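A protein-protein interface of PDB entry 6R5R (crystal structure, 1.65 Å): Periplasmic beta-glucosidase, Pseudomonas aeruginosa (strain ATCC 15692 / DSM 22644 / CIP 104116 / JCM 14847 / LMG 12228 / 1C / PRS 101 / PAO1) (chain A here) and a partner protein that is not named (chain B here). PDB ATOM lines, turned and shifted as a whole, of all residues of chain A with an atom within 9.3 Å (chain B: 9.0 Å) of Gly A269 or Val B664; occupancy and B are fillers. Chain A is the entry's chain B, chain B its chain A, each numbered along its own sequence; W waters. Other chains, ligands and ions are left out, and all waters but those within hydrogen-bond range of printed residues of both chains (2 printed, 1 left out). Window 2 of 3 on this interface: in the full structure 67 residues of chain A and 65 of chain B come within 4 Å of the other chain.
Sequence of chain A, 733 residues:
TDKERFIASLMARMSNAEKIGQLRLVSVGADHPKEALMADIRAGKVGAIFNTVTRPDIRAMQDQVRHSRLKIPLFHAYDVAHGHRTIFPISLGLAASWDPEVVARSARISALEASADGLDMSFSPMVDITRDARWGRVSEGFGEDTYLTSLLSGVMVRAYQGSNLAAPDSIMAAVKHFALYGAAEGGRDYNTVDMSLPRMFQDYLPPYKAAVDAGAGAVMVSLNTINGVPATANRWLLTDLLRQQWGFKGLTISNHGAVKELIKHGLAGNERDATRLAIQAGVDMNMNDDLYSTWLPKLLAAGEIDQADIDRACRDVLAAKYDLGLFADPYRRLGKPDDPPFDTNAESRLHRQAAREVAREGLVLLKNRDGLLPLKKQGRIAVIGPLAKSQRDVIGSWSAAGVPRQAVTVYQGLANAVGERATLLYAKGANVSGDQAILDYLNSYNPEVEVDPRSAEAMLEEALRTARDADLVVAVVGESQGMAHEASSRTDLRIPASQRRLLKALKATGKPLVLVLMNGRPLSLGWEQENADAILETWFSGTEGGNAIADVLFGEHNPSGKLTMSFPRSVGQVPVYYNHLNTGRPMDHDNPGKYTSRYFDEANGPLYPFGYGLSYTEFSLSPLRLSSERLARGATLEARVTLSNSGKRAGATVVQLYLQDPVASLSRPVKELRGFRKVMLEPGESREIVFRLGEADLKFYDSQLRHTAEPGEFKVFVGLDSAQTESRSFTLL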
ATOM      1  N   VAL A 259     -19.905   1.811  -7.113  1.00  0.00           N
ATOM      2  CA  VAL A 259     -19.115   0.912  -7.997  1.00  0.00           C
ATOM      3  C   VAL A 259     -19.481   1.240  -9.451  1.00  0.00           C
ATOM      4  O   VAL A 259     -18.589   1.452 -10.304  1.00  0.00           O
ATOM      5  CB  VAL A 259     -19.345  -0.569  -7.652  1.00  0.00           C
ATOM      6  CG1 VAL A 259     -18.608  -1.456  -8.657  1.00  0.00           C
ATOM      7  CG2 VAL A 259     -18.938  -0.847  -6.214  1.00  0.00           C
ATOM      8  N   LYS A 260     -20.768   1.316  -9.763  1.00  0.00           N
ATOM      9  CA  LYS A 260     -21.192   1.667 -11.141  1.00  0.00           C
ATOM     10  C   LYS A 260     -20.677   3.065 -11.560  1.00  0.00           C
ATOM     11  O   LYS A 260     -20.337   3.291 -12.754  1.00  0.00           O
ATOM     12  CB  LYS A 260     -22.719   1.552 -11.196  1.00  0.00           C
ATOM     13  CG  LYS A 260     -23.258   1.681 -12.595  1.00  0.00           C
ATOM     14  CD  LYS A 260     -24.773   1.429 -12.626  1.00  0.00           C
ATOM     15  CE  LYS A 260     -25.373   1.830 -13.952  1.00  0.00           C
ATOM     16  NZ  LYS A 260     -26.699   1.199 -14.174  1.00  0.00           N
ATOM     17  N   GLU A 261     -20.601   4.019 -10.612  1.00  0.00           N
ATOM     18  CA  GLU A 261     -20.109   5.385 -10.903  1.00  0.00           C
ATOM     19  C   GLU A 261     -18.647   5.397 -11.371  1.00  0.00           C
ATOM     20  O   GLU A 261     -18.219   6.412 -11.936  1.00  0.00           O
ATOM     21  CB  GLU A 261     -20.285   6.334  -9.714  1.00  0.00           C
ATOM     22  CG  GLU A 261     -21.729   6.690  -9.459  1.00  0.00           C
ATOM     23  CD  GLU A 261     -21.943   7.607  -8.251  1.00  0.00           C
ATOM     24  OE1 GLU A 261     -20.985   8.314  -7.842  1.00  0.00           O
ATOM     25  OE2 GLU A 261     -23.081   7.601  -7.700  1.00  0.00           O
ATOM     26  N   LEU A 262     -17.871   4.333 -11.152  1.00  0.00           N
ATOM     27  CA  LEU A 262     -16.487   4.310 -11.707  1.00  0.00           C
ATOM     28  C   LEU A 262     -16.490   4.525 -13.222  1.00  0.00           C
ATOM     29  O   LEU A 262     -15.463   4.948 -13.787  1.00  0.00           O
ATOM     30  CB  LEU A 262     -15.792   3.007 -11.296  1.00  0.00           C
ATOM     31  CG  LEU A 262     -15.540   2.900  -9.804  1.00  0.00           C
ATOM     32  CD1 LEU A 262     -14.959   1.528  -9.466  1.00  0.00           C
ATOM     33  CD2 LEU A 262     -14.582   3.966  -9.271  1.00  0.00           C
ATOM     34  N   ILE A 263     -17.594   4.182 -13.918  1.00  0.00           N
ATOM     35  CA  ILE A 263     -17.695   4.390 -15.380  1.00  0.00           C
ATOM     36  C   ILE A 263     -17.784   5.905 -15.682  1.00  0.00           C
ATOM     37  O   ILE A 263     -17.042   6.405 -16.508  1.00  0.00           O
ATOM     38  CB  ILE A 263     -18.905   3.621 -15.921  1.00  0.00           C
ATOM     39  CG1 ILE A 263     -18.754   2.117 -15.668  1.00  0.00           C
ATOM     40  CG2 ILE A 263     -19.083   3.992 -17.377  1.00  0.00           C
ATOM     41  CD1 ILE A 263     -20.016   1.323 -15.960  1.00  0.00           C
ATOM     42  N   LYS A 264     -18.624   6.630 -14.949  1.00  0.00           N
ATOM     43  CA  LYS A 264     -18.757   8.090 -15.113  1.00  0.00           C
ATOM     44  C   LYS A 264     -17.436   8.768 -14.752  1.00  0.00           C
ATOM     45  O   LYS A 264     -17.077   9.761 -15.401  1.00  0.00           O
ATOM     46  CB  LYS A 264     -19.917   8.652 -14.293  1.00  0.00           C
ATOM     47  CG  LYS A 264     -21.294   8.096 -14.645  1.00  0.00           C
ATOM     48  CD  LYS A 264     -21.898   8.601 -15.900  1.00  0.00           C
ATOM     49  CE  LYS A 264     -23.389   8.282 -15.971  1.00  0.00           C
ATOM     50  NZ  LYS A 264     -24.208   9.151 -15.067  1.00  0.00           N
ATOM     51  N   HIS A 265     -16.739   8.281 -13.736  1.00  0.00           N
ATOM     52  CA  HIS A 265     -15.426   8.851 -13.369  1.00  0.00           C
ATOM     53  C   HIS A 265     -14.395   8.585 -14.460  1.00  0.00           C
ATOM     54  O   HIS A 265     -13.306   9.209 -14.422  1.00  0.00           O
ATOM     55  CB  HIS A 265     -14.928   8.280 -12.067  1.00  0.00           C
ATOM     56  CG  HIS A 265     -15.506   8.833 -10.821  1.00  0.00           C
ATOM     57  ND1 HIS A 265     -15.221  10.113 -10.402  1.00  0.00           N
ATOM     58  CD2 HIS A 265     -16.274   8.262  -9.861  1.00  0.00           C
ATOM     59  CE1 HIS A 265     -15.769  10.257  -9.190  1.00  0.00           C
ATOM     60  NE2 HIS A 265     -16.427   9.168  -8.860  1.00  0.00           N
ATOM     61  N   GLY A 266     -14.660   7.674 -15.403  1.00  0.00           N
ATOM     62  CA  GLY A 266     -13.625   7.381 -16.414  1.00  0.00           C
ATOM     63  C   GLY A 266     -12.511   6.473 -15.937  1.00  0.00           C
ATOM     64  O   GLY A 266     -11.431   6.524 -16.569  1.00  0.00           O
ATOM     65  N   LEU A 267     -12.777   5.615 -14.957  1.00  0.00           N
ATOM     66  CA  LEU A 267     -11.821   4.583 -14.511  1.00  0.00           C
ATOM     67  C   LEU A 267     -12.155   3.254 -15.192  1.00  0.00           C
ATOM     68  O   LEU A 267     -11.332   2.347 -15.188  1.00  0.00           O
ATOM     69  CB  LEU A 267     -11.874   4.424 -12.991  1.00  0.00           C
ATOM     70  CG  LEU A 267     -10.848   5.217 -12.171  1.00  0.00           C
ATOM     71  CD1 LEU A 267      -9.477   4.604 -12.247  1.00  0.00           C
ATOM     72  CD2 LEU A 267     -10.795   6.686 -12.594  1.00  0.00           C
ATOM     73  N   ALA A 268     -13.389   3.116 -15.675  1.00  0.00           N
ATOM     74  CA  ALA A 268     -13.838   1.833 -16.269  1.00  0.00           C
ATOM     75  C   ALA A 268     -14.721   2.143 -17.454  1.00  0.00           C
ATOM     76  O   ALA A 268     -15.399   3.146 -17.439  1.00  0.00           O
ATOM     77  CB  ALA A 268     -14.592   1.059 -15.230  1.00  0.00           C
ATOM     78  N   GLY A 269     -14.736   1.276 -18.460  1.00  0.00           N
ATOM     79  CA  GLY A 269     -15.612   1.501 -19.615  1.00  0.00           C
ATOM     80  C   GLY A 269     -16.865   0.654 -19.536  1.00  0.00           C
ATOM     81  O   GLY A 269     -17.753   0.804 -20.383  1.00  0.00           O
ATOM     82  N   ASN A 270     -16.925  -0.227 -18.558  1.00  0.00           N
ATOM     83  CA  ASN A 270     -18.089  -1.115 -18.399  1.00  0.00           C
ATOM     84  C   ASN A 270     -18.222  -1.558 -16.945  1.00  0.00           C
ATOM     85  O   ASN A 270     -17.278  -1.397 -16.125  1.00  0.00           O
ATOM     86  CB  ASN A 270     -17.979  -2.290 -19.368  1.00  0.00           C
ATOM     87  CG  ASN A 270     -16.709  -3.062 -19.161  1.00  0.00           C
ATOM     88  OD1 ASN A 270     -16.487  -3.637 -18.109  1.00  0.00           O
ATOM     89  ND2 ASN A 270     -15.800  -2.981 -20.119  1.00  0.00           N
ATOM     90  N   GLU A 271     -19.338  -2.194 -16.636  1.00  0.00           N
ATOM     91  CA  GLU A 271     -19.615  -2.607 -15.242  1.00  0.00           C
ATOM     92  C   GLU A 271     -18.693  -3.737 -14.782  1.00  0.00           C
ATOM     93  O   GLU A 271     -18.406  -3.830 -13.601  1.00  0.00           O
ATOM     94  CB  GLU A 271     -21.047  -3.087 -15.131  1.00  0.00           C
ATOM     95  CG  GLU A 271     -22.055  -1.999 -15.324  1.00  0.00           C
ATOM     96  CD  GLU A 271     -23.451  -2.544 -15.106  1.00  0.00           C
ATOM     97  OE1 GLU A 271     -23.624  -3.783 -14.841  1.00  0.00           O
ATOM     98  OE2 GLU A 271     -24.346  -1.753 -15.186  1.00  0.00           O
ATOM     99  N   ARG A 272     -18.251  -4.637 -15.662  1.00  0.00           N
ATOM    100  CA  ARG A 272     -17.347  -5.746 -15.292  1.00  0.00           C
ATOM    101  C   ARG A 272     -16.029  -5.169 -14.753  1.00  0.00           C
ATOM    102  O   ARG A 272     -15.523  -5.594 -13.730  1.00  0.00           O
ATOM    103  CB  ARG A 272     -17.169  -6.604 -16.550  1.00  0.00           C
ATOM    104  CG  ARG A 272     -16.210  -7.759 -16.412  1.00  0.00           C
ATOM    105  CD  ARG A 272     -16.161  -8.528 -17.737  1.00  0.00           C
ATOM    106  NE  ARG A 272     -15.389  -9.740 -17.514  1.00  0.00           N
ATOM    107  CZ  ARG A 272     -15.738 -10.976 -17.911  1.00  0.00           C
ATOM    108  NH1 ARG A 272     -16.833 -11.193 -18.640  1.00  0.00           N
ATOM    109  NH2 ARG A 272     -14.928 -11.976 -17.618  1.00  0.00           N
ATOM    110  N   ASP A 273     -15.474  -4.199 -15.479  1.00  0.00           N
ATOM    111  CA  ASP A 273     -14.168  -3.593 -15.084  1.00  0.00           C
ATOM    112  C   ASP A 273     -14.375  -2.742 -13.821  1.00  0.00           C
ATOM    113  O   ASP A 273     -13.492  -2.750 -12.974  1.00  0.00           O
ATOM    114  CB  ASP A 273     -13.584  -2.798 -16.240  1.00  0.00           C
ATOM    115  CG  ASP A 273     -13.111  -3.702 -17.381  1.00  0.00           C
ATOM    116  OD1 ASP A 273     -12.894  -4.950 -17.155  1.00  0.00           O
ATOM    117  OD2 ASP A 273     -12.973  -3.182 -18.489  1.00  0.00           O
ATOM    118  N   ALA A 274     -15.510  -2.082 -13.686  1.00  0.00           N
ATOM    119  CA  ALA A 274     -15.787  -1.310 -12.447  1.00  0.00           C
ATOM    120  C   ALA A 274     -15.782  -2.244 -11.238  1.00  0.00           C
ATOM    121  O   ALA A 274     -15.174  -1.947 -10.164  1.00  0.00           O
ATOM    122  CB  ALA A 274     -17.072  -0.559 -12.564  1.00  0.00           C
ATOM    123  N   THR A 275     -16.468  -3.391 -11.376  1.00  0.00           N
ATOM    124  CA  THR A 275     -16.568  -4.364 -10.286  1.00  0.00           C
ATOM    125  C   THR A 275     -15.168  -4.826  -9.864  1.00  0.00           C
ATOM    126  O   THR A 275     -14.851  -4.908  -8.662  1.00  0.00           O
ATOM    127  CB  THR A 275     -17.427  -5.550 -10.742  1.00  0.00           C
ATOM    128  OG1 THR A 275     -18.738  -5.065 -10.995  1.00  0.00           O
ATOM    129  CG2 THR A 275     -17.484  -6.623  -9.668  1.00  0.00           C
ATOM    130  N   ARG A 276     -14.331  -5.169 -10.857  1.00  0.00           N
ATOM    131  CA  ARG A 276     -12.969  -5.664 -10.586  1.00  0.00           C
ATOM    132  C   ARG A 276     -12.189  -4.598  -9.801  1.00  0.00           C
ATOM    133  O   ARG A 276     -11.530  -4.940  -8.790  1.00  0.00           O
ATOM    134  CB  ARG A 276     -12.258  -5.998 -11.895  1.00  0.00           C
ATOM    135  CG  ARG A 276     -10.848  -6.481 -11.618  1.00  0.00           C
ATOM    136  CD  ARG A 276      -9.948  -6.571 -12.822  1.00  0.00           C
ATOM    137  NE  ARG A 276      -9.242  -5.321 -13.015  1.00  0.00           N
ATOM    138  CZ  ARG A 276      -9.371  -4.537 -14.083  1.00  0.00           C
ATOM    139  NH1 ARG A 276      -8.659  -3.427 -14.156  1.00  0.00           N
ATOM    140  NH2 ARG A 276     -10.209  -4.860 -15.063  1.00  0.00           N
ATOM    141  N   LEU A 277     -12.286  -3.350 -10.237  1.00  0.00           N
ATOM    142  CA  LEU A 277     -11.523  -2.269  -9.581  1.00  0.00           C
ATOM    143  C   LEU A 277     -11.950  -2.165  -8.129  1.00  0.00           C
ATOM    144  O   LEU A 277     -11.087  -2.024  -7.254  1.00  0.00           O
ATOM    145  CB  LEU A 277     -11.746  -0.954 -10.319  1.00  0.00           C
ATOM    146  CG  LEU A 277     -11.053  -0.843 -11.678  1.00  0.00           C
ATOM    147  CD1 LEU A 277     -11.462   0.435 -12.395  1.00  0.00           C
ATOM    148  CD2 LEU A 277      -9.549  -0.896 -11.506  1.00  0.00           C
ATOM    149  N   GLN B 661     -10.297  13.752 -25.331  1.00  0.00           N
ATOM    150  CA  GLN B 661     -10.740  13.131 -24.070  1.00  0.00           C
ATOM    151  C   GLN B 661     -10.214  11.698 -24.036  1.00  0.00           C
ATOM    152  O   GLN B 661     -10.269  11.035 -25.093  1.00  0.00           O
ATOM    153  CB  GLN B 661     -12.259  13.127 -23.932  1.00  0.00           C
ATOM    154  CG  GLN B 661     -12.729  12.486 -22.630  1.00  0.00           C
ATOM    155  CD  GLN B 661     -14.214  12.353 -22.520  1.00  0.00           C
ATOM    156  OE1 GLN B 661     -14.903  12.532 -23.501  1.00  0.00           O
ATOM    157  NE2 GLN B 661     -14.705  12.124 -21.308  1.00  0.00           N
ATOM    158  N   ASP B 662      -9.754  11.250 -22.867  1.00  0.00           N
ATOM    159  CA  ASP B 662      -9.303   9.857 -22.638  1.00  0.00           C
ATOM    160  C   ASP B 662     -10.313   9.242 -21.685  1.00  0.00           C
ATOM    161  O   ASP B 662     -10.169   9.407 -20.455  1.00  0.00           O
ATOM    162  CB  ASP B 662      -7.887   9.848 -22.124  1.00  0.00           C
ATOM    163  CG  ASP B 662      -7.300   8.492 -21.867  1.00  0.00           C
ATOM    164  OD1 ASP B 662      -8.020   7.489 -22.103  1.00  0.00           O
ATOM    165  OD2 ASP B 662      -6.159   8.479 -21.357  1.00  0.00           O
ATOM    166  N   PRO B 663     -11.419   8.673 -22.190  1.00  0.00           N
ATOM    167  CA  PRO B 663     -12.567   8.400 -21.320  1.00  0.00           C
ATOM    168  C   PRO B 663     -12.421   7.216 -20.368  1.00  0.00           C
ATOM    169  O   PRO B 663     -13.263   7.065 -19.486  1.00  0.00           O
ATOM    170  CB  PRO B 663     -13.702   8.135 -22.308  1.00  0.00           C
ATOM    171  CG  PRO B 663     -13.000   7.602 -23.518  1.00  0.00           C
ATOM    172  CD  PRO B 663     -11.732   8.419 -23.606  1.00  0.00           C
ATOM    173  N   VAL B 664     -11.399   6.376 -20.538  1.00  0.00           N
ATOM    174  CA  VAL B 664     -11.102   5.294 -19.576  1.00  0.00           C
ATOM    175  C   VAL B 664      -9.616   5.326 -19.284  1.00  0.00           C
ATOM    176  O   VAL B 664      -8.831   5.241 -20.214  1.00  0.00           O
ATOM    177  CB  VAL B 664     -11.512   3.911 -20.117  1.00  0.00           C
ATOM    178  CG1 VAL B 664     -11.154   2.835 -19.104  1.00  0.00           C
ATOM    179  CG2 VAL B 664     -13.002   3.861 -20.505  1.00  0.00           C
ATOM    180  N   ALA B 665      -9.219   5.509 -18.043  1.00  0.00           N
ATOM    181  CA  ALA B 665      -7.788   5.651 -17.733  1.00  0.00           C
ATOM    182  C   ALA B 665      -7.545   5.262 -16.286  1.00  0.00           C
ATOM    183  O   ALA B 665      -8.525   5.092 -15.512  1.00  0.00           O
ATOM    184  CB  ALA B 665      -7.358   7.070 -18.016  1.00  0.00           C
ATOM    185  N   SER B 666      -6.293   5.121 -15.918  1.00  0.00           N
ATOM    186  CA  SER B 666      -5.917   4.719 -14.547  1.00  0.00           C
ATOM    187  C   SER B 666      -5.984   5.899 -13.566  1.00  0.00           C
ATOM    188  O   SER B 666      -5.824   5.651 -12.403  1.00  0.00           O
ATOM    189  CB  SER B 666      -4.572   4.059 -14.510  1.00  0.00           C
ATOM    190  OG  SER B 666      -3.597   4.938 -15.015  1.00  0.00           O
ATOM    191  N   LEU B 667      -6.278   7.104 -14.034  1.00  0.00           N
ATOM    192  CA  LEU B 667      -6.706   8.294 -13.267  1.00  0.00           C
ATOM    193  C   LEU B 667      -7.979   8.805 -13.949  1.00  0.00           C
ATOM    194  O   LEU B 667      -8.090   8.680 -15.166  1.00  0.00           O
ATOM    195  CB  LEU B 667      -5.646   9.413 -13.403  1.00  0.00           C
ATOM    196  CG  LEU B 667      -4.553   9.590 -12.365  1.00  0.00           C
ATOM    197  CD1 LEU B 667      -4.115  11.033 -12.334  1.00  0.00           C
ATOM    198  CD2 LEU B 667      -4.970   9.135 -10.992  1.00  0.00           C
ATOM    199  N   SER B 668      -8.835   9.514 -13.249  1.00  0.00           N
ATOM    200  CA  SER B 668      -9.981  10.211 -13.869  1.00  0.00           C
ATOM    201  C   SER B 668      -9.453  11.389 -14.710  1.00  0.00           C
ATOM    202  O   SER B 668      -8.841  12.278 -14.142  1.00  0.00           O
ATOM    203  CB  SER B 668     -10.942  10.658 -12.801  1.00  0.00           C
ATOM    204  OG  SER B 668     -12.110  11.220 -13.347  1.00  0.00           O
ATOM    205  N   ARG B 669      -9.629  11.372 -16.027  1.00  0.00           N
ATOM    206  CA  ARG B 669      -9.093  12.399 -16.907  1.00  0.00           C
ATOM    207  C   ARG B 669     -10.170  13.431 -17.240  1.00  0.00           C
ATOM    208  O   ARG B 669     -11.397  13.155 -17.192  1.00  0.00           O
ATOM    209  CB  ARG B 669      -8.561  11.745 -18.189  1.00  0.00           C
ATOM    210  CG  ARG B 669      -7.510  10.668 -17.908  1.00  0.00           C
ATOM    211  CD  ARG B 669      -6.170  11.321 -17.748  1.00  0.00           C
ATOM    212  NE  ARG B 669      -5.678  11.886 -19.001  1.00  0.00           N
ATOM    213  CZ  ARG B 669      -5.245  13.130 -19.212  1.00  0.00           C
ATOM    214  NH1 ARG B 669      -5.142  14.066 -18.252  1.00  0.00           N
ATOM    215  NH2 ARG B 669      -4.877  13.412 -20.444  1.00  0.00           N
ATOM    216  N   PRO B 670      -9.733  14.639 -17.589  1.00  0.00           N
ATOM    217  CA  PRO B 670     -10.680  15.709 -17.880  1.00  0.00           C
ATOM    218  C   PRO B 670     -11.653  15.369 -18.995  1.00  0.00           C
ATOM    219  O   PRO B 670     -11.358  14.554 -19.898  1.00  0.00           O
ATOM    220  CB  PRO B 670      -9.832  16.891 -18.299  1.00  0.00           C
ATOM    221  CG  PRO B 670      -8.530  16.626 -17.658  1.00  0.00           C
ATOM    222  CD  PRO B 670      -8.340  15.122 -17.646  1.00  0.00           C
ATOM    223  N   LEU B 699      -1.124  12.070 -26.227  1.00  0.00           N
ATOM    224  CA  LEU B 699      -2.083  11.168 -25.537  1.00  0.00           C
ATOM    225  C   LEU B 699      -1.596  10.800 -24.139  1.00  0.00           C
ATOM    226  O   LEU B 699      -2.313  10.090 -23.416  1.00  0.00           O
ATOM    227  CB  LEU B 699      -2.251   9.903 -26.389  1.00  0.00           C
ATOM    228  CG  LEU B 699      -2.633  10.128 -27.844  1.00  0.00           C
ATOM    229  CD1 LEU B 699      -2.810   8.792 -28.569  1.00  0.00           C
ATOM    230  CD2 LEU B 699      -3.877  10.974 -28.005  1.00  0.00           C
ATOM    231  N   PHE B 701      -0.356  11.115 -20.150  1.00  0.00           N
ATOM    232  CA  PHE B 701      -0.714  11.861 -18.918  1.00  0.00           C
ATOM    233  C   PHE B 701       0.068  11.295 -17.757  1.00  0.00           C
ATOM    234  O   PHE B 701       0.608  10.175 -17.809  1.00  0.00           O
ATOM    235  CB  PHE B 701      -2.213  11.737 -18.638  1.00  0.00           C
ATOM    236  CG  PHE B 701      -2.644  10.345 -18.233  1.00  0.00           C
ATOM    237  CD1 PHE B 701      -2.778   9.345 -19.186  1.00  0.00           C
ATOM    238  CD2 PHE B 701      -2.878  10.010 -16.920  1.00  0.00           C
ATOM    239  CE1 PHE B 701      -3.163   8.067 -18.834  1.00  0.00           C
ATOM    240  CE2 PHE B 701      -3.232   8.716 -16.554  1.00  0.00           C
ATOM    241  CZ  PHE B 701      -3.376   7.744 -17.512  1.00  0.00           C
ATOM    242  N   ALA B 710       1.071   6.960 -22.463  1.00  0.00           N
ATOM    243  CA  ALA B 710      -0.270   6.883 -23.075  1.00  0.00           C
ATOM    244  C   ALA B 710      -0.755   5.456 -22.929  1.00  0.00           C
ATOM    245  O   ALA B 710       0.003   4.510 -23.271  1.00  0.00           O
ATOM    246  CB  ALA B 710      -0.152   7.318 -24.489  1.00  0.00           C
ATOM    247  N   GLU B 711      -1.970   5.279 -22.409  1.00  0.00           N
ATOM    248  CA  GLU B 711      -2.535   3.936 -22.249  1.00  0.00           C
ATOM    249  C   GLU B 711      -3.347   3.576 -23.483  1.00  0.00           C
ATOM    250  O   GLU B 711      -4.065   4.400 -24.069  1.00  0.00           O
ATOM    251  CB  GLU B 711      -3.431   3.880 -21.025  1.00  0.00           C
ATOM    252  CG  GLU B 711      -2.704   4.184 -19.740  1.00  0.00           C
ATOM    253  CD  GLU B 711      -3.570   4.246 -18.481  1.00  0.00           C
ATOM    254  OE1 GLU B 711      -4.732   4.666 -18.587  1.00  0.00           O
ATOM    255  OE2 GLU B 711      -3.040   3.958 -17.382  1.00  0.00           O
ATOM    256  N   PRO B 712      -3.254   2.304 -23.935  1.00  0.00           N
ATOM    257  CA  PRO B 712      -4.068   1.883 -25.060  1.00  0.00           C
ATOM    258  C   PRO B 712      -5.547   2.032 -24.683  1.00  0.00           C
ATOM    259  O   PRO B 712      -5.903   1.905 -23.508  1.00  0.00           O
ATOM    260  CB  PRO B 712      -3.698   0.371 -25.223  1.00  0.00           C
ATOM    261  CG  PRO B 712      -3.168  -0.050 -23.875  1.00  0.00           C
ATOM    262  CD  PRO B 712      -2.512   1.202 -23.291  1.00  0.00           C
ATOM    263  N   GLY B 713      -6.365   2.209 -25.702  1.00  0.00           N
ATOM    264  CA  GLY B 713      -7.820   2.331 -25.578  1.00  0.00           C
ATOM    265  C   GLY B 713      -8.348   3.521 -26.315  1.00  0.00           C
ATOM    266  O   GLY B 713      -7.646   4.122 -27.166  1.00  0.00           O
ATOM    267  N   GLU B 714      -9.601   3.852 -26.038  1.00  0.00           N
ATOM    268  CA  GLU B 714     -10.308   4.867 -26.811  1.00  0.00           C
ATOM    269  C   GLU B 714      -9.792   6.272 -26.488  1.00  0.00           C
ATOM    270  O   GLU B 714      -9.501   6.570 -25.322  1.00  0.00           O
ATOM    271  CB  GLU B 714     -11.806   4.795 -26.526  1.00  0.00           C
ATOM    272  CG  GLU B 714     -12.641   5.809 -27.283  1.00  0.00           C
ATOM    273  CD  GLU B 714     -14.128   5.787 -26.952  1.00  0.00           C
ATOM    274  OE1 GLU B 714     -14.487   5.164 -25.937  1.00  0.00           O
ATOM    275  OE2 GLU B 714     -14.919   6.432 -27.681  1.00  0.00           O
ATOM    276  N   PHE B 715      -9.733   7.098 -27.490  1.00  0.00           N
ATOM    277  CA  PHE B 715      -9.600   8.574 -27.364  1.00  0.00           C
ATOM    278  C   PHE B 715     -10.711   9.206 -28.168  1.00  0.00           C
ATOM    279  O   PHE B 715     -11.014   8.769 -29.276  1.00  0.00           O
ATOM    280  CB  PHE B 715      -8.247   9.111 -27.817  1.00  0.00           C
ATOM    281  CG  PHE B 715      -7.135   8.669 -26.925  1.00  0.00           C
ATOM    282  CD1 PHE B 715      -6.542   7.422 -27.094  1.00  0.00           C
ATOM    283  CD2 PHE B 715      -6.739   9.460 -25.857  1.00  0.00           C
ATOM    284  CE1 PHE B 715      -5.517   7.018 -26.278  1.00  0.00           C
ATOM    285  CE2 PHE B 715      -5.788   8.995 -24.973  1.00  0.00           C
ATOM    286  CZ  PHE B 715      -5.165   7.795 -25.177  1.00  0.00           C
ATOM    287  N   LYS B 716     -11.317  10.244 -27.625  1.00  0.00           N
ATOM    288  CA  LYS B 716     -12.319  11.028 -28.324  1.00  0.00           C
ATOM    289  C   LYS B 716     -11.688  12.339 -28.782  1.00  0.00           C
ATOM    290  O   LYS B 716     -11.035  13.019 -27.968  1.00  0.00           O
ATOM    291  CB  LYS B 716     -13.507  11.271 -27.411  1.00  0.00           C
ATOM    292  CG  LYS B 716     -14.228  10.002 -26.994  1.00  0.00           C
ATOM    293  CD  LYS B 716     -15.396  10.244 -26.073  1.00  0.00           C
ATOM    294  CE  LYS B 716     -16.267  11.373 -26.556  1.00  0.00           C
ATOM    295  NZ  LYS B 716     -16.606  11.269 -27.998  1.00  0.00           N
HETATM  296  O   HOH W   1     -10.808   9.089 -17.684  1.00  0.00           O
HETATM  297  O   HOH W   2     -14.156  12.319 -11.792  1.00  0.00           O
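Of the printed residues of chain B, Gly A266 touches Pro B663, Val B664 and Ala B665. Printed residues of chain B within 4 Å of Leu A267: Val B664, Ala B665, Ser B666, Leu B667 and Ser B668. Of chain B, only Val B664 (3.9 Å) comes within 4 Å of Ala A268. Gly A269 touches one residue of chain B. No residue of chain B comes within 4 Å of Asn A270. Arg A276 touches none of the printed residues of chain B. Asp B662 touches none of the printed residues of chain A. Of chain A, only Gly A266 (3.1 Å) comes within 4 Å of Pro B663. Of chain A, only Gly A266 (3.3 Å), Leu A267 (3.95 Å), Ala A268 (3.9 Å) and Gly A269 (3.6 Å) come within 4 Å of Val B664. Printed residues of chain A within 4 Å of Ala B665: Gly A266 (2.8 Å) and Leu A267 (3.4 Å). Printed residues of chain A within 4 Å of Ser B666: Leu A267. Of the printed residues of chain A, Ser B668 touches His A265 and Leu A267. The nearest residue of chain B that does not touch Gly A269 is Pro B663 (6.0 Å).
Water W2 lies within hydrogen-bond range of the side-chain hydroxyl of Ser B668 (2.8 Å) and a ring nitrogen (ND1) of His A265 (2.8 Å). Water W1 lies within hydrogen-bond range of the backbone carbonyl oxygen of Asp B662 (2.9 Å), the backbone carbonyl oxygen of Gly A266 (2.9 Å) and the backbone NH of Arg B669 (3.1 Å).
O of His A265 is in hydrogen-bond range of OG of Ser B668 (2.6 Å). The backbone carbonyl oxygen (O) of Gly A266 lies within hydrogen-bond range of the backbone NH (N) of Ala B665. O of Gly A266 sits close to O of Pro B663, 3.5 Å away.
The backbone NH of Leu A267 sits at hydrogen-bond distance from the backbone carbonyl oxygen of Leu A262 (3.0 Å). N of Ala A268 is in hydrogen-bond range of O of Leu A262 (3.3 Å). OG of Ser B666 is in hydrogen-bond range of OE2 of Glu B711 (2.6 Å).
Among the printed residues, pairs that only touch across the chains: Gly A266 with Val B664 (3.3 Å), Leu A267 with Val B664 (3.95 Å), Leu A267 with Ala B665 (3.4 Å), Leu A267 with Ser B666 (3.8 Å), Leu A267 with Leu B667 (3.8 Å), Leu A267 with Ser B668 (3.5 Å), Ala A268 with Val B664 (3.9 Å) and Gly A269 with Val B664 (3.6 Å).
Of the 19 printed residues of chain A, 5 touch a printed residue of chain B. Hydrophobic or aromatic side chains of chain A within 4 Å of the printed part of chain B: Leu A267. Hydrophobic or aromatic side chains of chain B that line the printed part of chain A: Val B664.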
